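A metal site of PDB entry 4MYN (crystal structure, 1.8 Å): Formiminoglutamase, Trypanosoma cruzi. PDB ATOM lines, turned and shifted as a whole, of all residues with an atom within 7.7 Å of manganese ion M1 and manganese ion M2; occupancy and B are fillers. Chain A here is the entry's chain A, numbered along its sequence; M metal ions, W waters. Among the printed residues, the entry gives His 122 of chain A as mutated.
Manganese ion M2 is bound by OD1 of Asp 146 (2.2 Å), water W2 (2.2 Å), ND1 of His 148 (2.2 Å), OD2 of Asp 236 (2.2 Å), OD1 of Asp 238 (2.3 Å) and OD2 of Asp 238 (2.4 Å).
Ser 147 touches manganese ion M2.
Along chain A the residues within 4 Å of manganese ion M2 span positions 146 to 238.
The nearest printed residue that does not touch manganese ion M2 is Asp 150 (4.5 Å).
Manganese ion M1 is bound by the side-chain carboxylate (OD2) of Asp 146, the side-chain carboxylate (OD2) of Asp 236, a ring nitrogen (ND1) of His 122, the side-chain carboxylate (OD2) of Asp 150, water W2 and water W1.
Water W1 bridges the backbone carbonyl oxygen (O) of Ser 162 (2.9 Å) and the side-chain carboxylate (OE2) of Glu 281 (3.3 Å).
NE2 of His 148 sits close to OG of Ser 147.
A ring nitrogen (NE2) of His 148 sits at hydrogen-bond distance from the side-chain sulfur (SG) of Cys 250, at 3.4 Å.
A ring nitrogen (NE2) of His 148 lies within hydrogen-bond range of the side-chain amide oxygen of Gln 189.
The backbone carbonyl oxygen (O) of Asp 236 is in hydrogen-bond range of the side-chain hydroxyl (OG) of Ser 239, at 2.9 Å.
O of Val 145 is in hydrogen-bond range of N of Asp 236 (2.7 Å).
The side-chain carboxylate of Glu 281 lies within hydrogen-bond range of the backbone NH of His 122, 2.8 Å away.
The backbone NH (N) of Phe 166 is in hydrogen-bond range of the backbone carbonyl oxygen (O) of Asp 150 (3.2 Å).
The backbone carbonyl oxygen (O) of Asp 238 sits at hydrogen-bond distance from the side-chain hydroxyl (OG) of Ser 147.
Four residues have an atom within 4 Å of manganese ion M1: His 122, Asp 146, Asp 150 and Asp 236.
The nearest printed residue that does not touch manganese ion M1 is Ser 162 (4.2 Å).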
ATOM      1  N   ASN A  46      26.160  30.996   1.578  1.00  0.00           N
ATOM      2  CA  ASN A  46      25.122  31.834   0.959  1.00  0.00           C
ATOM      3  C   ASN A  46      24.199  32.409   2.040  1.00  0.00           C
ATOM      4  O   ASN A  46      23.071  32.822   1.761  1.00  0.00           O
ATOM      5  CB  ASN A  46      24.326  31.000  -0.050  1.00  0.00           C
ATOM      6  CG  ASN A  46      23.378  31.836  -0.900  1.00  0.00           C
ATOM      7  OD1 ASN A  46      23.652  33.008  -1.204  1.00  0.00           O
ATOM      8  ND2 ASN A  46      22.256  31.235  -1.299  1.00  0.00           N
ATOM      9  N   GLY A 121      23.126  20.974  -0.177  1.00  0.00           N
ATOM     10  CA  GLY A 121      22.928  22.306  -0.732  1.00  0.00           C
ATOM     11  C   GLY A 121      22.845  22.318  -2.247  1.00  0.00           C
ATOM     12  O   GLY A 121      23.365  21.421  -2.906  1.00  0.00           O
ATOM     13  N   HIS A 122      22.233  23.358  -2.796  1.00  0.00           N
ATOM     14  CA  HIS A 122      22.020  23.452  -4.233  1.00  0.00           C
ATOM     15  C   HIS A 122      23.300  23.672  -5.035  1.00  0.00           C
ATOM     16  O   HIS A 122      23.288  23.570  -6.261  1.00  0.00           O
ATOM     17  CB  HIS A 122      21.026  24.573  -4.559  1.00  0.00           C
ATOM     18  CG  HIS A 122      20.230  24.339  -5.807  1.00  0.00           C
ATOM     19  ND1 HIS A 122      19.193  25.148  -6.198  1.00  0.00           N
ATOM     20  CD2 HIS A 122      20.330  23.363  -6.753  1.00  0.00           C
ATOM     21  CE1 HIS A 122      18.684  24.701  -7.333  1.00  0.00           C
ATOM     22  NE2 HIS A 122      19.351  23.609  -7.683  1.00  0.00           N
ATOM     23  N   ASP A 123      24.401  23.977  -4.349  1.00  0.00           N
ATOM     24  CA  ASP A 123      25.688  24.081  -5.040  1.00  0.00           C
ATOM     25  C   ASP A 123      26.047  22.814  -5.840  1.00  0.00           C
ATOM     26  O   ASP A 123      26.844  22.881  -6.788  1.00  0.00           O
ATOM     27  CB  ASP A 123      26.825  24.464  -4.086  1.00  0.00           C
ATOM     28  CG  ASP A 123      26.802  23.666  -2.789  1.00  0.00           C
ATOM     29  OD1 ASP A 123      25.869  23.902  -1.959  1.00  0.00           O
ATOM     30  OD2 ASP A 123      27.716  22.834  -2.585  1.00  0.00           O
ATOM     31  N   SER A 125      24.451  21.477  -8.014  1.00  0.00           N
ATOM     32  CA  SER A 125      23.963  21.564  -9.388  1.00  0.00           C
ATOM     33  C   SER A 125      25.034  22.015 -10.379  1.00  0.00           C
ATOM     34  O   SER A 125      24.904  21.761 -11.572  1.00  0.00           O
ATOM     35  CB  SER A 125      22.729  22.455  -9.462  1.00  0.00           C
ATOM     36  OG  SER A 125      21.680  21.828  -8.756  1.00  0.00           O
ATOM     37  N   ASN A 144      15.808  24.984 -13.647  1.00  0.00           N
ATOM     38  CA  ASN A 144      15.981  25.138 -12.218  1.00  0.00           C
ATOM     39  C   ASN A 144      14.627  25.438 -11.580  1.00  0.00           C
ATOM     40  O   ASN A 144      14.089  26.541 -11.730  1.00  0.00           O
ATOM     41  CB  ASN A 144      16.965  26.260 -11.902  1.00  0.00           C
ATOM     42  CG  ASN A 144      17.141  26.489 -10.415  1.00  0.00           C
ATOM     43  OD1 ASN A 144      17.060  25.553  -9.622  1.00  0.00           O
ATOM     44  ND2 ASN A 144      17.341  27.730 -10.024  1.00  0.00           N
ATOM     45  N   VAL A 145      14.075  24.450 -10.864  1.00  0.00           N
ATOM     46  CA  VAL A 145      12.820  24.661 -10.149  1.00  0.00           C
ATOM     47  C   VAL A 145      13.209  25.192  -8.773  1.00  0.00           C
ATOM     48  O   VAL A 145      13.762  24.455  -7.944  1.00  0.00           O
ATOM     49  CB  VAL A 145      11.986  23.373  -9.981  1.00  0.00           C
ATOM     50  CG1 VAL A 145      10.641  23.697  -9.284  1.00  0.00           C
ATOM     51  CG2 VAL A 145      11.744  22.710 -11.355  1.00  0.00           C
ATOM     52  N   ASP A 146      12.932  26.468  -8.564  1.00  0.00           N
ATOM     53  CA  ASP A 146      13.497  27.180  -7.427  1.00  0.00           C
ATOM     54  C   ASP A 146      12.740  28.477  -7.204  1.00  0.00           C
ATOM     55  O   ASP A 146      12.412  29.189  -8.166  1.00  0.00           O
ATOM     56  CB  ASP A 146      14.968  27.481  -7.774  1.00  0.00           C
ATOM     57  CG  ASP A 146      15.799  27.812  -6.559  1.00  0.00           C
ATOM     58  OD1 ASP A 146      15.248  28.290  -5.552  1.00  0.00           O
ATOM     59  OD2 ASP A 146      17.030  27.598  -6.650  1.00  0.00           O
ATOM     60  N   SER A 147      12.456  28.828  -5.959  1.00  0.00           N
ATOM     61  CA  SER A 147      11.932  30.173  -5.692  1.00  0.00           C
ATOM     62  C   SER A 147      12.985  31.251  -6.004  1.00  0.00           C
ATOM     63  O   SER A 147      12.635  32.409  -6.238  1.00  0.00           O
ATOM     64  CB  SER A 147      11.427  30.302  -4.257  1.00  0.00           C
ATOM     65  OG  SER A 147      12.430  29.918  -3.339  1.00  0.00           O
ATOM     66  N   HIS A 148      14.253  30.868  -5.999  1.00  0.00           N
ATOM     67  CA  HIS A 148      15.369  31.797  -6.217  1.00  0.00           C
ATOM     68  C   HIS A 148      16.073  31.545  -7.563  1.00  0.00           C
ATOM     69  O   HIS A 148      15.998  30.461  -8.077  1.00  0.00           O
ATOM     70  CB  HIS A 148      16.394  31.654  -5.095  1.00  0.00           C
ATOM     71  CG  HIS A 148      15.761  31.532  -3.744  1.00  0.00           C
ATOM     72  ND1 HIS A 148      15.559  30.308  -3.119  1.00  0.00           N
ATOM     73  CD2 HIS A 148      15.275  32.477  -2.905  1.00  0.00           C
ATOM     74  CE1 HIS A 148      14.980  30.521  -1.949  1.00  0.00           C
ATOM     75  NE2 HIS A 148      14.788  31.819  -1.794  1.00  0.00           N
ATOM     76  N   LEU A 149      16.788  32.543  -8.095  1.00  0.00           N
ATOM     77  CA  LEU A 149      17.436  32.367  -9.404  1.00  0.00           C
ATOM     78  C   LEU A 149      18.797  31.660  -9.316  1.00  0.00           C
ATOM     79  O   LEU A 149      19.207  30.938 -10.252  1.00  0.00           O
ATOM     80  CB  LEU A 149      17.614  33.721 -10.115  1.00  0.00           C
ATOM     81  CG  LEU A 149      16.368  34.488 -10.553  1.00  0.00           C
ATOM     82  CD1 LEU A 149      16.815  35.649 -11.427  1.00  0.00           C
ATOM     83  CD2 LEU A 149      15.428  33.582 -11.317  1.00  0.00           C
ATOM     84  N   ASP A 150      19.486  31.866  -8.206  1.00  0.00           N
ATOM     85  CA  ASP A 150      20.748  31.173  -7.938  1.00  0.00           C
ATOM     86  C   ASP A 150      21.803  31.481  -9.000  1.00  0.00           C
ATOM     87  O   ASP A 150      22.505  30.578  -9.468  1.00  0.00           O
ATOM     88  CB  ASP A 150      20.534  29.665  -7.836  1.00  0.00           C
ATOM     89  CG  ASP A 150      19.925  29.264  -6.506  1.00  0.00           C
ATOM     90  OD1 ASP A 150      19.303  30.130  -5.843  1.00  0.00           O
ATOM     91  OD2 ASP A 150      20.092  28.083  -6.126  1.00  0.00           O
ATOM     92  N   SER A 162      25.552  27.893  -2.351  1.00  0.00           N
ATOM     93  CA  SER A 162      24.219  27.432  -2.744  1.00  0.00           C
ATOM     94  C   SER A 162      23.481  28.406  -3.680  1.00  0.00           C
ATOM     95  O   SER A 162      22.411  28.085  -4.194  1.00  0.00           O
ATOM     96  CB  SER A 162      23.360  27.067  -1.506  1.00  0.00           C
ATOM     97  OG  SER A 162      23.060  28.199  -0.706  1.00  0.00           O
ATOM     98  N   GLY A 163      24.057  29.578  -3.896  1.00  0.00           N
ATOM     99  CA  GLY A 163      23.414  30.584  -4.734  1.00  0.00           C
ATOM    100  C   GLY A 163      24.120  30.879  -6.048  1.00  0.00           C
ATOM    101  O   GLY A 163      23.675  31.748  -6.797  1.00  0.00           O
ATOM    102  N   THR A 164      25.204  30.160  -6.334  1.00  0.00           N
ATOM    103  CA  THR A 164      25.961  30.401  -7.569  1.00  0.00           C
ATOM    104  C   THR A 164      25.856  29.354  -8.691  1.00  0.00           C
ATOM    105  O   THR A 164      26.369  29.608  -9.770  1.00  0.00           O
ATOM    106  CB  THR A 164      27.453  30.586  -7.277  1.00  0.00           C
ATOM    107  OG1 THR A 164      28.000  29.340  -6.837  1.00  0.00           O
ATOM    108  CG2 THR A 164      27.659  31.644  -6.197  1.00  0.00           C
ATOM    109  N   PRO A 165      25.191  28.212  -8.445  1.00  0.00           N
ATOM    110  CA  PRO A 165      25.383  27.096  -9.390  1.00  0.00           C
ATOM    111  C   PRO A 165      25.016  27.402 -10.838  1.00  0.00           C
ATOM    112  O   PRO A 165      25.620  26.841 -11.760  1.00  0.00           O
ATOM    113  CB  PRO A 165      24.430  25.999  -8.869  1.00  0.00           C
ATOM    114  CG  PRO A 165      23.885  26.499  -7.582  1.00  0.00           C
ATOM    115  CD  PRO A 165      24.098  27.960  -7.495  1.00  0.00           C
ATOM    116  N   PHE A 166      24.031  28.271 -11.048  1.00  0.00           N
ATOM    117  CA  PHE A 166      23.582  28.533 -12.422  1.00  0.00           C
ATOM    118  C   PHE A 166      24.280  29.725 -13.048  1.00  0.00           C
ATOM    119  O   PHE A 166      24.175  29.961 -14.246  1.00  0.00           O
ATOM    120  CB  PHE A 166      22.059  28.587 -12.499  1.00  0.00           C
ATOM    121  CG  PHE A 166      21.428  27.312 -12.041  1.00  0.00           C
ATOM    122  CD1 PHE A 166      21.383  26.210 -12.870  1.00  0.00           C
ATOM    123  CD2 PHE A 166      20.992  27.184 -10.727  1.00  0.00           C
ATOM    124  CE1 PHE A 166      20.854  25.009 -12.422  1.00  0.00           C
ATOM    125  CE2 PHE A 166      20.458  25.991 -10.274  1.00  0.00           C
ATOM    126  CZ  PHE A 166      20.386  24.907 -11.119  1.00  0.00           C
ATOM    127  N   GLU A 182      14.299  29.149 -15.529  1.00  0.00           N
ATOM    128  CA  GLU A 182      14.139  29.336 -14.100  1.00  0.00           C
ATOM    129  C   GLU A 182      12.646  29.179 -13.838  1.00  0.00           C
ATOM    130  O   GLU A 182      11.851  30.017 -14.256  1.00  0.00           O
ATOM    131  CB  GLU A 182      14.612  30.714 -13.679  1.00  0.00           C
ATOM    132  CG  GLU A 182      16.125  30.987 -13.888  1.00  0.00           C
ATOM    133  CD  GLU A 182      16.978  30.644 -12.667  1.00  0.00           C
ATOM    134  OE1 GLU A 182      16.600  29.751 -11.873  1.00  0.00           O
ATOM    135  OE2 GLU A 182      18.060  31.273 -12.517  1.00  0.00           O
ATOM    136  N   GLN A 189      11.643  37.643  -4.154  1.00  0.00           N
ATOM    137  CA  GLN A 189      12.884  37.039  -3.677  1.00  0.00           C
ATOM    138  C   GLN A 189      13.969  37.072  -4.740  1.00  0.00           C
ATOM    139  O   GLN A 189      15.065  36.538  -4.518  1.00  0.00           O
ATOM    140  CB  GLN A 189      12.676  35.555  -3.319  1.00  0.00           C
ATOM    141  CG  GLN A 189      11.557  35.227  -2.362  1.00  0.00           C
ATOM    142  CD  GLN A 189      11.841  33.949  -1.601  1.00  0.00           C
ATOM    143  OE1 GLN A 189      12.851  33.842  -0.891  1.00  0.00           O
ATOM    144  NE2 GLN A 189      10.958  32.944  -1.736  1.00  0.00           N
ATOM    145  N   SER A 234      16.502  20.066 -12.261  1.00  0.00           N
ATOM    146  CA  SER A 234      17.112  20.441 -10.986  1.00  0.00           C
ATOM    147  C   SER A 234      16.047  21.037 -10.074  1.00  0.00           C
ATOM    148  O   SER A 234      15.468  22.078 -10.389  1.00  0.00           O
ATOM    149  CB  SER A 234      18.238  21.454 -11.199  1.00  0.00           C
ATOM    150  OG  SER A 234      18.925  21.746  -9.989  1.00  0.00           O
ATOM    151  N   PHE A 235      15.805  20.384  -8.947  1.00  0.00           N
ATOM    152  CA  PHE A 235      14.685  20.762  -8.091  1.00  0.00           C
ATOM    153  C   PHE A 235      15.195  21.237  -6.733  1.00  0.00           C
ATOM    154  O   PHE A 235      15.776  20.480  -5.974  1.00  0.00           O
ATOM    155  CB  PHE A 235      13.739  19.551  -7.908  1.00  0.00           C
ATOM    156  CG  PHE A 235      12.266  19.934  -7.762  1.00  0.00           C
ATOM    157  CD1 PHE A 235      11.873  20.883  -6.827  1.00  0.00           C
ATOM    158  CD2 PHE A 235      11.304  19.326  -8.551  1.00  0.00           C
ATOM    159  CE1 PHE A 235      10.510  21.217  -6.678  1.00  0.00           C
ATOM    160  CE2 PHE A 235       9.941  19.660  -8.402  1.00  0.00           C
ATOM    161  CZ  PHE A 235       9.554  20.616  -7.471  1.00  0.00           C
ATOM    162  N   ASP A 236      14.953  22.510  -6.437  1.00  0.00           N
ATOM    163  CA  ASP A 236      15.234  23.064  -5.107  1.00  0.00           C
ATOM    164  C   ASP A 236      13.919  23.023  -4.352  1.00  0.00           C
ATOM    165  O   ASP A 236      12.980  23.685  -4.747  1.00  0.00           O
ATOM    166  CB  ASP A 236      15.649  24.501  -5.248  1.00  0.00           C
ATOM    167  CG  ASP A 236      16.028  25.137  -3.923  1.00  0.00           C
ATOM    168  OD1 ASP A 236      15.664  24.623  -2.850  1.00  0.00           O
ATOM    169  OD2 ASP A 236      16.707  26.164  -3.963  1.00  0.00           O
ATOM    170  N   VAL A 237      13.859  22.237  -3.271  1.00  0.00           N
ATOM    171  CA  VAL A 237      12.580  22.011  -2.592  1.00  0.00           C
ATOM    172  C   VAL A 237      12.050  23.261  -1.861  1.00  0.00           C
ATOM    173  O   VAL A 237      10.902  23.276  -1.394  1.00  0.00           O
ATOM    174  CB  VAL A 237      12.587  20.762  -1.651  1.00  0.00           C
ATOM    175  CG1 VAL A 237      12.705  19.474  -2.461  1.00  0.00           C
ATOM    176  CG2 VAL A 237      13.644  20.882  -0.572  1.00  0.00           C
ATOM    177  N   ASP A 238      12.870  24.313  -1.786  1.00  0.00           N
ATOM    178  CA  ASP A 238      12.363  25.581  -1.262  1.00  0.00           C
ATOM    179  C   ASP A 238      11.501  26.347  -2.279  1.00  0.00           C
ATOM    180  O   ASP A 238      11.083  27.473  -2.021  1.00  0.00           O
ATOM    181  CB  ASP A 238      13.483  26.461  -0.661  1.00  0.00           C
ATOM    182  CG  ASP A 238      14.381  27.115  -1.712  1.00  0.00           C
ATOM    183  OD1 ASP A 238      13.969  27.315  -2.876  1.00  0.00           O
ATOM    184  OD2 ASP A 238      15.521  27.479  -1.324  1.00  0.00           O
ATOM    185  N   SER A 239      11.201  25.703  -3.415  1.00  0.00           N
ATOM    186  CA  SER A 239      10.208  26.216  -4.357  1.00  0.00           C
ATOM    187  C   SER A 239       8.807  25.833  -3.887  1.00  0.00           C
ATOM    188  O   SER A 239       7.828  26.399  -4.367  1.00  0.00           O
ATOM    189  CB  SER A 239      10.422  25.621  -5.762  1.00  0.00           C
ATOM    190  OG  SER A 239      10.278  24.201  -5.731  1.00  0.00           O
ATOM    191  N   CYS A 250      15.658  27.979   3.413  1.00  0.00           N
ATOM    192  CA  CYS A 250      14.934  29.220   3.141  1.00  0.00           C
ATOM    193  C   CYS A 250      13.460  28.896   2.877  1.00  0.00           C
ATOM    194  O   CYS A 250      13.059  28.801   1.722  1.00  0.00           O
ATOM    195  CB  CYS A 250      15.514  29.967   1.919  1.00  0.00           C
ATOM    196  SG  CYS A 250      14.792  31.648   1.591  1.00  0.00           S
ATOM    197  N   SER A 280      17.679  19.503  -4.016  1.00  0.00           N
ATOM    198  CA  SER A 280      18.549  20.220  -3.086  1.00  0.00           C
ATOM    199  C   SER A 280      17.745  20.965  -2.000  1.00  0.00           C
ATOM    200  O   SER A 280      16.560  21.249  -2.174  1.00  0.00           O
ATOM    201  CB  SER A 280      19.418  21.229  -3.844  1.00  0.00           C
ATOM    202  OG  SER A 280      20.187  20.582  -4.842  1.00  0.00           O
ATOM    203  N   GLU A 281      18.431  21.243  -0.902  1.00  0.00           N
ATOM    204  CA  GLU A 281      17.978  22.140   0.163  1.00  0.00           C
ATOM    205  C   GLU A 281      17.105  21.509   1.248  1.00  0.00           C
ATOM    206  O   GLU A 281      16.667  22.185   2.185  1.00  0.00           O
ATOM    207  CB  GLU A 281      17.363  23.438  -0.393  1.00  0.00           C
ATOM    208  CG  GLU A 281      18.359  24.239  -1.268  1.00  0.00           C
ATOM    209  CD  GLU A 281      19.541  24.792  -0.479  1.00  0.00           C
ATOM    210  OE1 GLU A 281      19.314  25.257   0.661  1.00  0.00           O
ATOM    211  OE2 GLU A 281      20.676  24.804  -1.006  1.00  0.00           O
HETATM  212 MN    MN M   1      18.458  26.933  -5.088  1.00  0.00          MN
HETATM  213 MN    MN M   2      16.004  28.205  -3.531  1.00  0.00          MN
HETATM  214  O   HOH W   1      19.844  27.101  -3.191  1.00  0.00           O
HETATM  215  O   HOH W   2      18.135  28.689  -3.654  1.00  0.00           O
